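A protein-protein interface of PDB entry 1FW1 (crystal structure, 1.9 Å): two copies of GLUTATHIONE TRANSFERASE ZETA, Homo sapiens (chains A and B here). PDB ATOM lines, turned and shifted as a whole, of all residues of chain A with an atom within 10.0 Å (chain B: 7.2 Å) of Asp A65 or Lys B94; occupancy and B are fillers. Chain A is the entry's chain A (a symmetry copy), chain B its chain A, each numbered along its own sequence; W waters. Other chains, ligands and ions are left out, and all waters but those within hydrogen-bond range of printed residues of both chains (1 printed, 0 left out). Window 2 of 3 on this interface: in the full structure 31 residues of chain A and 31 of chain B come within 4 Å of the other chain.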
ATOM      1  N   LYS A   5     -27.556  26.688   0.125  1.00  0.00           N
ATOM      2  CA  LYS A   5     -26.413  26.481   1.071  1.00  0.00           C
ATOM      3  C   LYS A   5     -26.482  25.061   1.626  1.00  0.00           C
ATOM      4  O   LYS A   5     -27.492  24.675   2.196  1.00  0.00           O
ATOM      5  CB  LYS A   5     -26.545  27.479   2.210  1.00  0.00           C
ATOM      6  CG  LYS A   5     -25.333  27.643   3.111  1.00  0.00           C
ATOM      7  CD  LYS A   5     -25.777  28.590   4.241  1.00  0.00           C
ATOM      8  CE  LYS A   5     -24.716  28.846   5.309  1.00  0.00           C
ATOM      9  NZ  LYS A   5     -25.319  29.572   6.491  1.00  0.00           N
ATOM     10  N   PRO A   6     -25.417  24.263   1.477  1.00  0.00           N
ATOM     11  CA  PRO A   6     -25.527  22.898   2.023  1.00  0.00           C
ATOM     12  C   PRO A   6     -25.660  22.832   3.544  1.00  0.00           C
ATOM     13  O   PRO A   6     -24.985  23.561   4.274  1.00  0.00           O
ATOM     14  CB  PRO A   6     -24.242  22.217   1.538  1.00  0.00           C
ATOM     15  CG  PRO A   6     -23.896  22.972   0.279  1.00  0.00           C
ATOM     16  CD  PRO A   6     -24.157  24.414   0.725  1.00  0.00           C
ATOM     17  N   ILE A   7     -26.524  21.944   4.010  1.00  0.00           N
ATOM     18  CA  ILE A   7     -26.735  21.766   5.420  1.00  0.00           C
ATOM     19  C   ILE A   7     -26.155  20.446   5.916  1.00  0.00           C
ATOM     20  O   ILE A   7     -26.537  19.382   5.432  1.00  0.00           O
ATOM     21  CB  ILE A   7     -28.243  21.714   5.810  1.00  0.00           C
ATOM     22  CG1 ILE A   7     -29.048  22.872   5.180  1.00  0.00           C
ATOM     23  CG2 ILE A   7     -28.351  21.775   7.336  1.00  0.00           C
ATOM     24  CD1 ILE A   7     -28.519  24.220   5.536  1.00  0.00           C
ATOM     25  N   LEU A  24     -15.627  18.899   3.252  1.00  0.00           N
ATOM     26  CA  LEU A  24     -16.275  20.122   2.832  1.00  0.00           C
ATOM     27  C   LEU A  24     -15.243  21.239   2.796  1.00  0.00           C
ATOM     28  O   LEU A  24     -15.250  22.056   1.888  1.00  0.00           O
ATOM     29  CB  LEU A  24     -17.434  20.455   3.784  1.00  0.00           C
ATOM     30  CG  LEU A  24     -18.612  19.496   3.605  1.00  0.00           C
ATOM     31  CD1 LEU A  24     -19.589  19.545   4.824  1.00  0.00           C
ATOM     32  CD2 LEU A  24     -19.353  19.885   2.326  1.00  0.00           C
ATOM     33  N   ILE A  29     -16.374  24.145   0.125  1.00  0.00           N
ATOM     34  CA  ILE A  29     -17.823  24.262   0.036  1.00  0.00           C
ATOM     35  C   ILE A  29     -18.358  24.861   1.343  1.00  0.00           C
ATOM     36  O   ILE A  29     -18.137  24.316   2.425  1.00  0.00           O
ATOM     37  CB  ILE A  29     -18.470  22.874  -0.186  1.00  0.00           C
ATOM     38  CG1 ILE A  29     -18.024  22.293  -1.536  1.00  0.00           C
ATOM     39  CG2 ILE A  29     -19.991  22.967  -0.148  1.00  0.00           C
ATOM     40  CD1 ILE A  29     -18.501  20.844  -1.704  1.00  0.00           C
ATOM     41  N   ASP A  30     -19.072  25.974   1.250  1.00  0.00           N
ATOM     42  CA  ASP A  30     -19.593  26.603   2.453  1.00  0.00           C
ATOM     43  C   ASP A  30     -20.815  25.872   2.916  1.00  0.00           C
ATOM     44  O   ASP A  30     -21.672  25.542   2.109  1.00  0.00           O
ATOM     45  CB  ASP A  30     -19.936  28.065   2.184  1.00  0.00           C
ATOM     46  CG  ASP A  30     -18.714  28.943   2.238  1.00  0.00           C
ATOM     47  OD1 ASP A  30     -17.912  28.758   3.201  1.00  0.00           O
ATOM     48  OD2 ASP A  30     -18.547  29.811   1.335  1.00  0.00           O
ATOM     49  N   LEU A  62     -26.133  14.896   5.138  1.00  0.00           N
ATOM     50  CA  LEU A  62     -25.867  16.143   4.436  1.00  0.00           C
ATOM     51  C   LEU A  62     -26.952  16.477   3.426  1.00  0.00           C
ATOM     52  O   LEU A  62     -27.318  15.618   2.625  1.00  0.00           O
ATOM     53  CB  LEU A  62     -24.547  16.079   3.676  1.00  0.00           C
ATOM     54  CG  LEU A  62     -24.179  17.355   2.920  1.00  0.00           C
ATOM     55  CD1 LEU A  62     -23.710  18.349   3.986  1.00  0.00           C
ATOM     56  CD2 LEU A  62     -23.062  17.128   1.875  1.00  0.00           C
ATOM     57  N   LYS A  63     -27.472  17.711   3.467  1.00  0.00           N
ATOM     58  CA  LYS A  63     -28.478  18.138   2.478  1.00  0.00           C
ATOM     59  C   LYS A  63     -27.683  18.982   1.500  1.00  0.00           C
ATOM     60  O   LYS A  63     -27.003  19.928   1.901  1.00  0.00           O
ATOM     61  CB  LYS A  63     -29.592  18.979   3.117  1.00  0.00           C
ATOM     62  CG  LYS A  63     -30.603  18.143   3.909  1.00  0.00           C
ATOM     63  CD  LYS A  63     -31.694  19.019   4.540  1.00  0.00           C
ATOM     64  CE  LYS A  63     -32.760  18.142   5.209  1.00  0.00           C
ATOM     65  NZ  LYS A  63     -33.811  18.906   5.973  1.00  0.00           N
ATOM     66  N   ILE A  64     -27.746  18.623   0.220  1.00  0.00           N
ATOM     67  CA  ILE A  64     -26.981  19.326  -0.793  1.00  0.00           C
ATOM     68  C   ILE A  64     -27.631  19.040  -2.145  1.00  0.00           C
ATOM     69  O   ILE A  64     -28.268  18.001  -2.327  1.00  0.00           O
ATOM     70  CB  ILE A  64     -25.482  18.849  -0.742  1.00  0.00           C
ATOM     71  CG1 ILE A  64     -24.624  19.685  -1.687  1.00  0.00           C
ATOM     72  CG2 ILE A  64     -25.405  17.321  -1.075  1.00  0.00           C
ATOM     73  CD1 ILE A  64     -23.115  19.537  -1.444  1.00  0.00           C
ATOM     74  N   ASP A  65     -27.528  19.994  -3.066  1.00  0.00           N
ATOM     75  CA  ASP A  65     -28.113  19.874  -4.406  1.00  0.00           C
ATOM     76  C   ASP A  65     -29.539  19.391  -4.383  1.00  0.00           C
ATOM     77  O   ASP A  65     -30.012  18.767  -5.336  1.00  0.00           O
ATOM     78  CB  ASP A  65     -27.276  18.940  -5.277  1.00  0.00           C
ATOM     79  CG  ASP A  65     -25.857  19.351  -5.303  1.00  0.00           C
ATOM     80  OD1 ASP A  65     -25.641  20.573  -5.107  1.00  0.00           O
ATOM     81  OD2 ASP A  65     -24.954  18.501  -5.518  1.00  0.00           O
ATOM     82  N   GLY A  66     -30.239  19.667  -3.291  1.00  0.00           N
ATOM     83  CA  GLY A  66     -31.629  19.261  -3.226  1.00  0.00           C
ATOM     84  C   GLY A  66     -31.884  17.842  -2.770  1.00  0.00           C
ATOM     85  O   GLY A  66     -33.011  17.373  -2.892  1.00  0.00           O
ATOM     86  N   ILE A  67     -30.867  17.133  -2.269  1.00  0.00           N
ATOM     87  CA  ILE A  67     -31.106  15.767  -1.810  1.00  0.00           C
ATOM     88  C   ILE A  67     -30.540  15.597  -0.419  1.00  0.00           C
ATOM     89  O   ILE A  67     -29.798  16.430   0.053  1.00  0.00           O
ATOM     90  CB  ILE A  67     -30.457  14.686  -2.732  1.00  0.00           C
ATOM     91  CG1 ILE A  67     -28.949  14.917  -2.857  1.00  0.00           C
ATOM     92  CG2 ILE A  67     -31.100  14.702  -4.112  1.00  0.00           C
ATOM     93  CD1 ILE A  67     -28.277  13.813  -3.642  1.00  0.00           C
ATOM     94  N   THR A  68     -30.895  14.502   0.228  1.00  0.00           N
ATOM     95  CA  THR A  68     -30.426  14.211   1.563  1.00  0.00           C
ATOM     96  C   THR A  68     -29.588  12.913   1.480  1.00  0.00           C
ATOM     97  O   THR A  68     -30.025  11.901   0.889  1.00  0.00           O
ATOM     98  CB  THR A  68     -31.651  14.098   2.502  1.00  0.00           C
ATOM     99  OG1 THR A  68     -32.246  15.413   2.611  1.00  0.00           O
ATOM    100  CG2 THR A  68     -31.258  13.654   3.912  1.00  0.00           C
ATOM    101  N   ILE A  69     -28.368  12.978   2.020  1.00  0.00           N
ATOM    102  CA  ILE A  69     -27.466  11.815   1.983  1.00  0.00           C
ATOM    103  C   ILE A  69     -26.949  11.470   3.350  1.00  0.00           C
ATOM    104  O   ILE A  69     -26.437  12.338   4.056  1.00  0.00           O
ATOM    105  CB  ILE A  69     -26.214  12.084   1.079  1.00  0.00           C
ATOM    106  CG1 ILE A  69     -26.649  12.622  -0.284  1.00  0.00           C
ATOM    107  CG2 ILE A  69     -25.398  10.721   0.841  1.00  0.00           C
ATOM    108  CD1 ILE A  69     -25.496  13.228  -1.027  1.00  0.00           C
ATOM    109  N   HIS A  70     -27.065  10.193   3.716  1.00  0.00           N
ATOM    110  CA  HIS A  70     -26.543   9.666   4.975  1.00  0.00           C
ATOM    111  C   HIS A  70     -25.325   8.811   4.596  1.00  0.00           C
ATOM    112  O   HIS A  70     -25.186   8.453   3.421  1.00  0.00           O
ATOM    113  CB  HIS A  70     -27.563   8.757   5.644  1.00  0.00           C
ATOM    114  CG  HIS A  70     -28.922   9.355   5.718  1.00  0.00           C
ATOM    115  ND1 HIS A  70     -29.159  10.574   6.321  1.00  0.00           N
ATOM    116  CD2 HIS A  70     -30.121   8.900   5.292  1.00  0.00           C
ATOM    117  CE1 HIS A  70     -30.451  10.839   6.273  1.00  0.00           C
ATOM    118  NE2 HIS A  70     -31.060   9.842   5.659  1.00  0.00           N
ATOM    119  N   ALA A  74     -20.360   7.665   1.685  1.00  0.00           N
ATOM    120  CA  ALA A  74     -21.192   7.885   0.522  1.00  0.00           C
ATOM    121  C   ALA A  74     -21.290   9.423   0.246  1.00  0.00           C
ATOM    122  O   ALA A  74     -21.361   9.865  -0.916  1.00  0.00           O
ATOM    123  CB  ALA A  74     -22.567   7.336   0.762  1.00  0.00           C
ATOM    124  N   ILE A  75     -21.253  10.214   1.316  1.00  0.00           N
ATOM    125  CA  ILE A  75     -21.342  11.683   1.204  1.00  0.00           C
ATOM    126  C   ILE A  75     -20.014  12.164   0.642  1.00  0.00           C
ATOM    127  O   ILE A  75     -19.955  12.945  -0.303  1.00  0.00           O
ATOM    128  CB  ILE A  75     -21.514  12.319   2.603  1.00  0.00           C
ATOM    129  CG1 ILE A  75     -22.936  12.046   3.117  1.00  0.00           C
ATOM    130  CG2 ILE A  75     -21.025  13.770   2.557  1.00  0.00           C
ATOM    131  CD1 ILE A  75     -23.099  12.395   4.653  1.00  0.00           C
ATOM    132  N   GLU A  77     -17.877  10.521  -1.178  1.00  0.00           N
ATOM    133  CA  GLU A  77     -17.727  10.206  -2.612  1.00  0.00           C
ATOM    134  C   GLU A  77     -18.671  11.053  -3.462  1.00  0.00           C
ATOM    135  O   GLU A  77     -18.369  11.365  -4.621  1.00  0.00           O
ATOM    136  CB  GLU A  77     -17.936   8.703  -2.904  1.00  0.00           C
ATOM    137  CG  GLU A  77     -16.863   7.866  -2.186  1.00  0.00           C
ATOM    138  CD  GLU A  77     -16.239   6.766  -3.078  1.00  0.00           C
ATOM    139  OE1 GLU A  77     -16.123   6.959  -4.316  1.00  0.00           O
ATOM    140  OE2 GLU A  77     -15.858   5.717  -2.519  1.00  0.00           O
ATOM    141  N   TYR A  78     -19.820  11.430  -2.918  1.00  0.00           N
ATOM    142  CA  TYR A  78     -20.722  12.289  -3.697  1.00  0.00           C
ATOM    143  C   TYR A  78     -20.034  13.639  -3.979  1.00  0.00           C
ATOM    144  O   TYR A  78     -20.104  14.164  -5.100  1.00  0.00           O
ATOM    145  CB  TYR A  78     -22.016  12.521  -2.943  1.00  0.00           C
ATOM    146  CG  TYR A  78     -22.930  13.440  -3.697  1.00  0.00           C
ATOM    147  CD1 TYR A  78     -23.655  12.992  -4.808  1.00  0.00           C
ATOM    148  CD2 TYR A  78     -23.041  14.791  -3.320  1.00  0.00           C
ATOM    149  CE1 TYR A  78     -24.474  13.876  -5.529  1.00  0.00           C
ATOM    150  CE2 TYR A  78     -23.858  15.690  -4.043  1.00  0.00           C
ATOM    151  CZ  TYR A  78     -24.560  15.243  -5.117  1.00  0.00           C
ATOM    152  OH  TYR A  78     -25.387  16.135  -5.770  1.00  0.00           O
ATOM    153  N   LEU A  79     -19.364  14.187  -2.968  1.00  0.00           N
ATOM    154  CA  LEU A  79     -18.634  15.448  -3.091  1.00  0.00           C
ATOM    155  C   LEU A  79     -17.446  15.333  -4.044  1.00  0.00           C
ATOM    156  O   LEU A  79     -17.123  16.278  -4.754  1.00  0.00           O
ATOM    157  CB  LEU A  79     -18.133  15.910  -1.718  1.00  0.00           C
ATOM    158  CG  LEU A  79     -19.207  16.185  -0.652  1.00  0.00           C
ATOM    159  CD1 LEU A  79     -18.498  16.543   0.646  1.00  0.00           C
ATOM    160  CD2 LEU A  79     -20.124  17.364  -1.103  1.00  0.00           C
ATOM    161  N   GLU A  80     -16.771  14.181  -4.039  1.00  0.00           N
ATOM    162  CA  GLU A  80     -15.650  13.969  -4.932  1.00  0.00           C
ATOM    163  C   GLU A  80     -16.129  13.958  -6.384  1.00  0.00           C
ATOM    164  O   GLU A  80     -15.458  14.553  -7.239  1.00  0.00           O
ATOM    165  CB  GLU A  80     -14.930  12.626  -4.592  1.00  0.00           C
ATOM    166  CG  GLU A  80     -13.919  12.170  -5.663  1.00  0.00           C
ATOM    167  CD  GLU A  80     -12.622  12.966  -5.638  1.00  0.00           C
ATOM    168  OE1 GLU A  80     -12.503  13.939  -4.845  1.00  0.00           O
ATOM    169  OE2 GLU A  80     -11.693  12.613  -6.421  1.00  0.00           O
ATOM    170  N   GLU A  81     -17.266  13.323  -6.672  1.00  0.00           N
ATOM    171  CA  GLU A  81     -17.821  13.254  -8.027  1.00  0.00           C
ATOM    172  C   GLU A  81     -18.469  14.572  -8.509  1.00  0.00           C
ATOM    173  O   GLU A  81     -18.433  14.871  -9.699  1.00  0.00           O
ATOM    174  CB  GLU A  81     -18.871  12.138  -8.134  1.00  0.00           C
ATOM    175  CG  GLU A  81     -18.242  10.713  -8.108  1.00  0.00           C
ATOM    176  CD  GLU A  81     -19.248   9.632  -7.879  1.00  0.00           C
ATOM    177  OE1 GLU A  81     -20.451   9.907  -8.005  1.00  0.00           O
ATOM    178  OE2 GLU A  81     -18.836   8.481  -7.570  1.00  0.00           O
ATOM    179  N   THR A  82     -19.043  15.350  -7.587  1.00  0.00           N
ATOM    180  CA  THR A  82     -19.686  16.580  -8.013  1.00  0.00           C
ATOM    181  C   THR A  82     -18.810  17.831  -8.008  1.00  0.00           C
ATOM    182  O   THR A  82     -19.087  18.736  -8.791  1.00  0.00           O
ATOM    183  CB  THR A  82     -21.013  16.820  -7.250  1.00  0.00           C
ATOM    184  OG1 THR A  82     -20.792  16.775  -5.842  1.00  0.00           O
ATOM    185  CG2 THR A  82     -22.009  15.753  -7.622  1.00  0.00           C
ATOM    186  N   ARG A  83     -17.782  17.881  -7.157  1.00  0.00           N
ATOM    187  CA  ARG A  83     -16.812  18.975  -7.090  1.00  0.00           C
ATOM    188  C   ARG A  83     -15.481  18.266  -7.224  1.00  0.00           C
ATOM    189  O   ARG A  83     -14.788  18.033  -6.228  1.00  0.00           O
ATOM    190  CB  ARG A  83     -16.852  19.674  -5.741  1.00  0.00           C
ATOM    191  CG  ARG A  83     -18.065  20.570  -5.594  1.00  0.00           C
ATOM    192  CD  ARG A  83     -19.337  19.772  -5.423  1.00  0.00           C
ATOM    193  NE  ARG A  83     -20.429  20.678  -5.106  1.00  0.00           N
ATOM    194  CZ  ARG A  83     -21.704  20.346  -4.962  1.00  0.00           C
ATOM    195  NH1 ARG A  83     -22.094  19.080  -5.093  1.00  0.00           N
ATOM    196  NH2 ARG A  83     -22.618  21.315  -4.727  1.00  0.00           N
ATOM    197  N   PRO B  90     -24.833   3.215 -10.902  1.00  0.00           N
ATOM    198  CA  PRO B  90     -25.427   3.984 -11.995  1.00  0.00           C
ATOM    199  C   PRO B  90     -24.495   5.103 -12.439  1.00  0.00           C
ATOM    200  O   PRO B  90     -23.426   5.307 -11.879  1.00  0.00           O
ATOM    201  CB  PRO B  90     -26.754   4.512 -11.400  1.00  0.00           C
ATOM    202  CG  PRO B  90     -26.469   4.559  -9.908  1.00  0.00           C
ATOM    203  CD  PRO B  90     -25.624   3.281  -9.674  1.00  0.00           C
ATOM    204  N   GLN B  91     -24.948   5.856 -13.429  1.00  0.00           N
ATOM    205  CA  GLN B  91     -24.212   6.975 -13.990  1.00  0.00           C
ATOM    206  C   GLN B  91     -24.408   8.291 -13.211  1.00  0.00           C
ATOM    207  O   GLN B  91     -23.479   9.049 -12.953  1.00  0.00           O
ATOM    208  CB  GLN B  91     -24.702   7.160 -15.428  1.00  0.00           C
ATOM    209  CG  GLN B  91     -23.738   7.826 -16.331  1.00  0.00           C
ATOM    210  CD  GLN B  91     -22.380   7.146 -16.316  1.00  0.00           C
ATOM    211  OE1 GLN B  91     -22.216   6.063 -15.729  1.00  0.00           O
ATOM    212  NE2 GLN B  91     -21.391   7.782 -16.942  1.00  0.00           N
ATOM    213  N   ASP B  92     -25.636   8.573 -12.868  1.00  0.00           N
ATOM    214  CA  ASP B  92     -25.960   9.820 -12.147  1.00  0.00           C
ATOM    215  C   ASP B  92     -25.455   9.848 -10.696  1.00  0.00           C
ATOM    216  O   ASP B  92     -25.816   8.983  -9.880  1.00  0.00           O
ATOM    217  CB  ASP B  92     -27.462  10.005 -12.226  1.00  0.00           C
ATOM    218  CG  ASP B  92     -27.984  10.982 -11.213  1.00  0.00           C
ATOM    219  OD1 ASP B  92     -27.200  11.841 -10.756  1.00  0.00           O
ATOM    220  OD2 ASP B  92     -29.191  10.873 -10.883  1.00  0.00           O
ATOM    221  N   PRO B  93     -24.630  10.858 -10.350  1.00  0.00           N
ATOM    222  CA  PRO B  93     -24.085  10.977  -9.000  1.00  0.00           C
ATOM    223  C   PRO B  93     -25.055  10.862  -7.833  1.00  0.00           C
ATOM    224  O   PRO B  93     -24.684  10.291  -6.800  1.00  0.00           O
ATOM    225  CB  PRO B  93     -23.347  12.303  -9.031  1.00  0.00           C
ATOM    226  CG  PRO B  93     -22.930  12.429 -10.477  1.00  0.00           C
ATOM    227  CD  PRO B  93     -24.172  11.980 -11.196  1.00  0.00           C
ATOM    228  N   LYS B  94     -26.287  11.372  -7.985  1.00  0.00           N
ATOM    229  CA  LYS B  94     -27.279  11.283  -6.906  1.00  0.00           C
ATOM    230  C   LYS B  94     -27.746   9.828  -6.731  1.00  0.00           C
ATOM    231  O   LYS B  94     -28.004   9.369  -5.617  1.00  0.00           O
ATOM    232  CB  LYS B  94     -28.501  12.207  -7.181  1.00  0.00           C
ATOM    233  CG  LYS B  94     -28.110  13.655  -7.508  1.00  0.00           C
ATOM    234  CD  LYS B  94     -29.332  14.620  -7.664  1.00  0.00           C
ATOM    235  CE  LYS B  94     -28.808  16.010  -8.121  1.00  0.00           C
ATOM    236  NZ  LYS B  94     -29.821  17.129  -8.061  1.00  0.00           N
ATOM    237  N   LYS B  95     -27.856   9.092  -7.823  1.00  0.00           N
ATOM    238  CA  LYS B  95     -28.252   7.694  -7.694  1.00  0.00           C
ATOM    239  C   LYS B  95     -27.042   6.887  -7.169  1.00  0.00           C
ATOM    240  O   LYS B  95     -27.209   5.913  -6.438  1.00  0.00           O
ATOM    241  CB  LYS B  95     -28.748   7.168  -9.023  1.00  0.00           C
ATOM    242  CG  LYS B  95     -30.052   7.846  -9.455  1.00  0.00           C
ATOM    243  CD  LYS B  95     -30.337   7.600 -10.937  1.00  0.00           C
ATOM    244  CE  LYS B  95     -31.432   8.549 -11.482  1.00  0.00           C
ATOM    245  NZ  LYS B  95     -31.350   8.701 -12.989  1.00  0.00           N
ATOM    246  N   ARG B  96     -25.833   7.330  -7.493  1.00  0.00           N
ATOM    247  CA  ARG B  96     -24.641   6.635  -6.994  1.00  0.00           C
ATOM    248  C   ARG B  96     -24.565   6.856  -5.489  1.00  0.00           C
ATOM    249  O   ARG B  96     -24.149   5.978  -4.743  1.00  0.00           O
ATOM    250  CB  ARG B  96     -23.377   7.141  -7.703  1.00  0.00           C
ATOM    251  CG  ARG B  96     -23.369   6.714  -9.179  1.00  0.00           C
ATOM    252  CD  ARG B  96     -22.288   7.427 -10.028  1.00  0.00           C
ATOM    253  NE  ARG B  96     -20.914   7.175  -9.621  1.00  0.00           N
ATOM    254  CZ  ARG B  96     -20.150   6.194 -10.129  1.00  0.00           C
ATOM    255  NH1 ARG B  96     -20.638   5.351 -11.040  1.00  0.00           N
ATOM    256  NH2 ARG B  96     -18.859   6.157  -9.831  1.00  0.00           N
ATOM    257  N   ALA B  97     -25.032   8.010  -5.022  1.00  0.00           N
ATOM    258  CA  ALA B  97     -24.992   8.249  -3.591  1.00  0.00           C
ATOM    259  C   ALA B  97     -26.027   7.364  -2.878  1.00  0.00           C
ATOM    260  O   ALA B  97     -25.771   6.872  -1.775  1.00  0.00           O
ATOM    261  CB  ALA B  97     -25.191   9.767  -3.267  1.00  0.00           C
ATOM    262  N   SER B  98     -27.169   7.114  -3.499  1.00  0.00           N
ATOM    263  CA  SER B  98     -28.147   6.215  -2.888  1.00  0.00           C
ATOM    264  C   SER B  98     -27.521   4.788  -2.790  1.00  0.00           C
ATOM    265  O   SER B  98     -27.672   4.124  -1.769  1.00  0.00           O
ATOM    266  CB  SER B  98     -29.428   6.094  -3.729  1.00  0.00           C
ATOM    267  OG  SER B  98     -30.065   7.353  -3.883  1.00  0.00           O
ATOM    268  N   VAL B  99     -26.865   4.323  -3.856  1.00  0.00           N
ATOM    269  CA  VAL B  99     -26.231   2.984  -3.842  1.00  0.00           C
ATOM    270  C   VAL B  99     -25.197   2.895  -2.735  1.00  0.00           C
ATOM    271  O   VAL B  99     -25.205   1.943  -1.946  1.00  0.00           O
ATOM    272  CB  VAL B  99     -25.510   2.666  -5.179  1.00  0.00           C
ATOM    273  CG1 VAL B  99     -24.622   1.353  -5.041  1.00  0.00           C
ATOM    274  CG2 VAL B  99     -26.550   2.499  -6.268  1.00  0.00           C
ATOM    275  N   MET B 101     -24.848   4.780  -0.044  1.00  0.00           N
ATOM    276  CA  MET B 101     -25.436   4.949   1.267  1.00  0.00           C
ATOM    277  C   MET B 101     -26.052   3.638   1.702  1.00  0.00           C
ATOM    278  O   MET B 101     -25.877   3.233   2.832  1.00  0.00           O
ATOM    279  CB  MET B 101     -26.540   6.058   1.226  1.00  0.00           C
ATOM    280  CG  MET B 101     -27.592   5.910   2.332  1.00  0.00           C
ATOM    281  SD  MET B 101     -28.716   7.401   2.378  1.00  0.00           S
ATOM    282  CE  MET B 101     -29.702   7.068   0.877  1.00  0.00           C
ATOM    283  N   THR B 149     -35.833   5.251  -2.740  1.00  0.00           N
ATOM    284  CA  THR B 149     -34.893   4.905  -3.827  1.00  0.00           C
ATOM    285  C   THR B 149     -35.228   3.737  -4.735  1.00  0.00           C
ATOM    286  O   THR B 149     -34.808   3.706  -5.910  1.00  0.00           O
ATOM    287  CB  THR B 149     -33.524   4.579  -3.249  1.00  0.00           C
ATOM    288  OG1 THR B 149     -33.631   3.356  -2.501  1.00  0.00           O
ATOM    289  CG2 THR B 149     -33.063   5.694  -2.311  1.00  0.00           C
ATOM    290  N   VAL B 155     -31.951   0.515  -5.876  1.00  0.00           N
ATOM    291  CA  VAL B 155     -31.860   1.864  -6.425  1.00  0.00           C
ATOM    292  C   VAL B 155     -32.288   1.756  -7.886  1.00  0.00           C
ATOM    293  O   VAL B 155     -31.558   1.234  -8.717  1.00  0.00           O
ATOM    294  CB  VAL B 155     -30.417   2.450  -6.335  1.00  0.00           C
ATOM    295  CG1 VAL B 155     -30.381   3.898  -6.917  1.00  0.00           C
ATOM    296  CG2 VAL B 155     -29.936   2.441  -4.892  1.00  0.00           C
HETATM  297  O   HOH W   1     -22.121  10.067  -5.761  1.00  0.00           O
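The side-chain amino group of Lys B94 is in hydrogen-bond range of the backbone carbonyl oxygen of Asp A65.
The side-chain sulfur of Met B101 lies within hydrogen-bond range of the backbone NH of His A70 (3.5 Å).
The side-chain carboxylate (OE2) of Glu A81 is in salt-bridge range of the guanidinium group (NE) of Arg B96 (3.2 Å).
O of Tyr A78 lies within hydrogen-bond range of OG1 of Thr A82 (2.8 Å).
The side-chain hydroxyl of Ser B98 is in hydrogen-bond range of the backbone carbonyl oxygen of Lys B94.
The backbone NH (N) of Lys B94 lies within hydrogen-bond range of the side-chain carboxylate (OD1) of Asp B92 (3.0 Å).
OG1 of Thr A82 is in hydrogen-bond range of NH1 of Arg A83.
OH of Tyr A78 lies within hydrogen-bond range of OD2 of Asp A65, at 2.4 Å.
OD2 of Asp A65 lies within salt-bridge range of NH1 of Arg A83, at 2.9 Å.
Among the printed residues, pairs that only touch across the chains: Ile A67 with Lys B94 (3.9 Å), Ala A74 with Met B101 (3.5 Å), Tyr A78 with Pro B93 (3.5 Å), Tyr A78 with Lys B94 (3.9 Å), Tyr A78 with Ala B97 (3.9 Å), Glu A81 with Pro B93 (3.9 Å) and Thr A82 with Pro B93 (3.96 Å).
Asp A65 touches just one residue of chain B: Lys B94.
Of the printed residues of chain A, Lys B94 touches Asp A65 (3.2 Å), Ile A67 (3.9 Å) and Tyr A78 (3.9 Å).
Pro B93 touches just these residues of chain A: Tyr A78, Glu A81 and Thr A82.
Of chain A, only Tyr A78 comes within 4 Å of Ala B97.
Of the printed residues of chain B, Tyr A78 touches Pro B93 (3.5 Å), Lys B94 (3.9 Å) and Ala B97 (3.9 Å).
Of the printed residues of chain A, Arg B96 touches Glu A81 (3.2 Å).
The nearest printed residue of chain B that does not touch Asp A65 is Pro B93 (7.3 Å).
The nearest printed residue of chain A that does not touch Met B101 is Ile A69 (4.5 Å).
Of the 24 printed residues of chain A, 7 touch a printed residue of chain B.
Of the 13 printed residues of chain B, 5 touch a printed residue of chain A.
Hydrophobic or aromatic side chains of chain B that line the printed part of chain A: Pro B93, Ala B97 and Met B101.
Among the printed residues, 10 pairs touch across the chains.
Among the printed residues, Asp or Glu carboxylates within 4 Å of a Lys or Arg side-chain nitrogen of the other chain: Glu A81 with Arg B96.
No position is printed for both chains.
Of the 10 pairs that touch across the chains among the printed residues, none has its exchanged pair printed and touching as well.
Water W1 bridges O of Pro B93 and OE1 of Glu A81.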
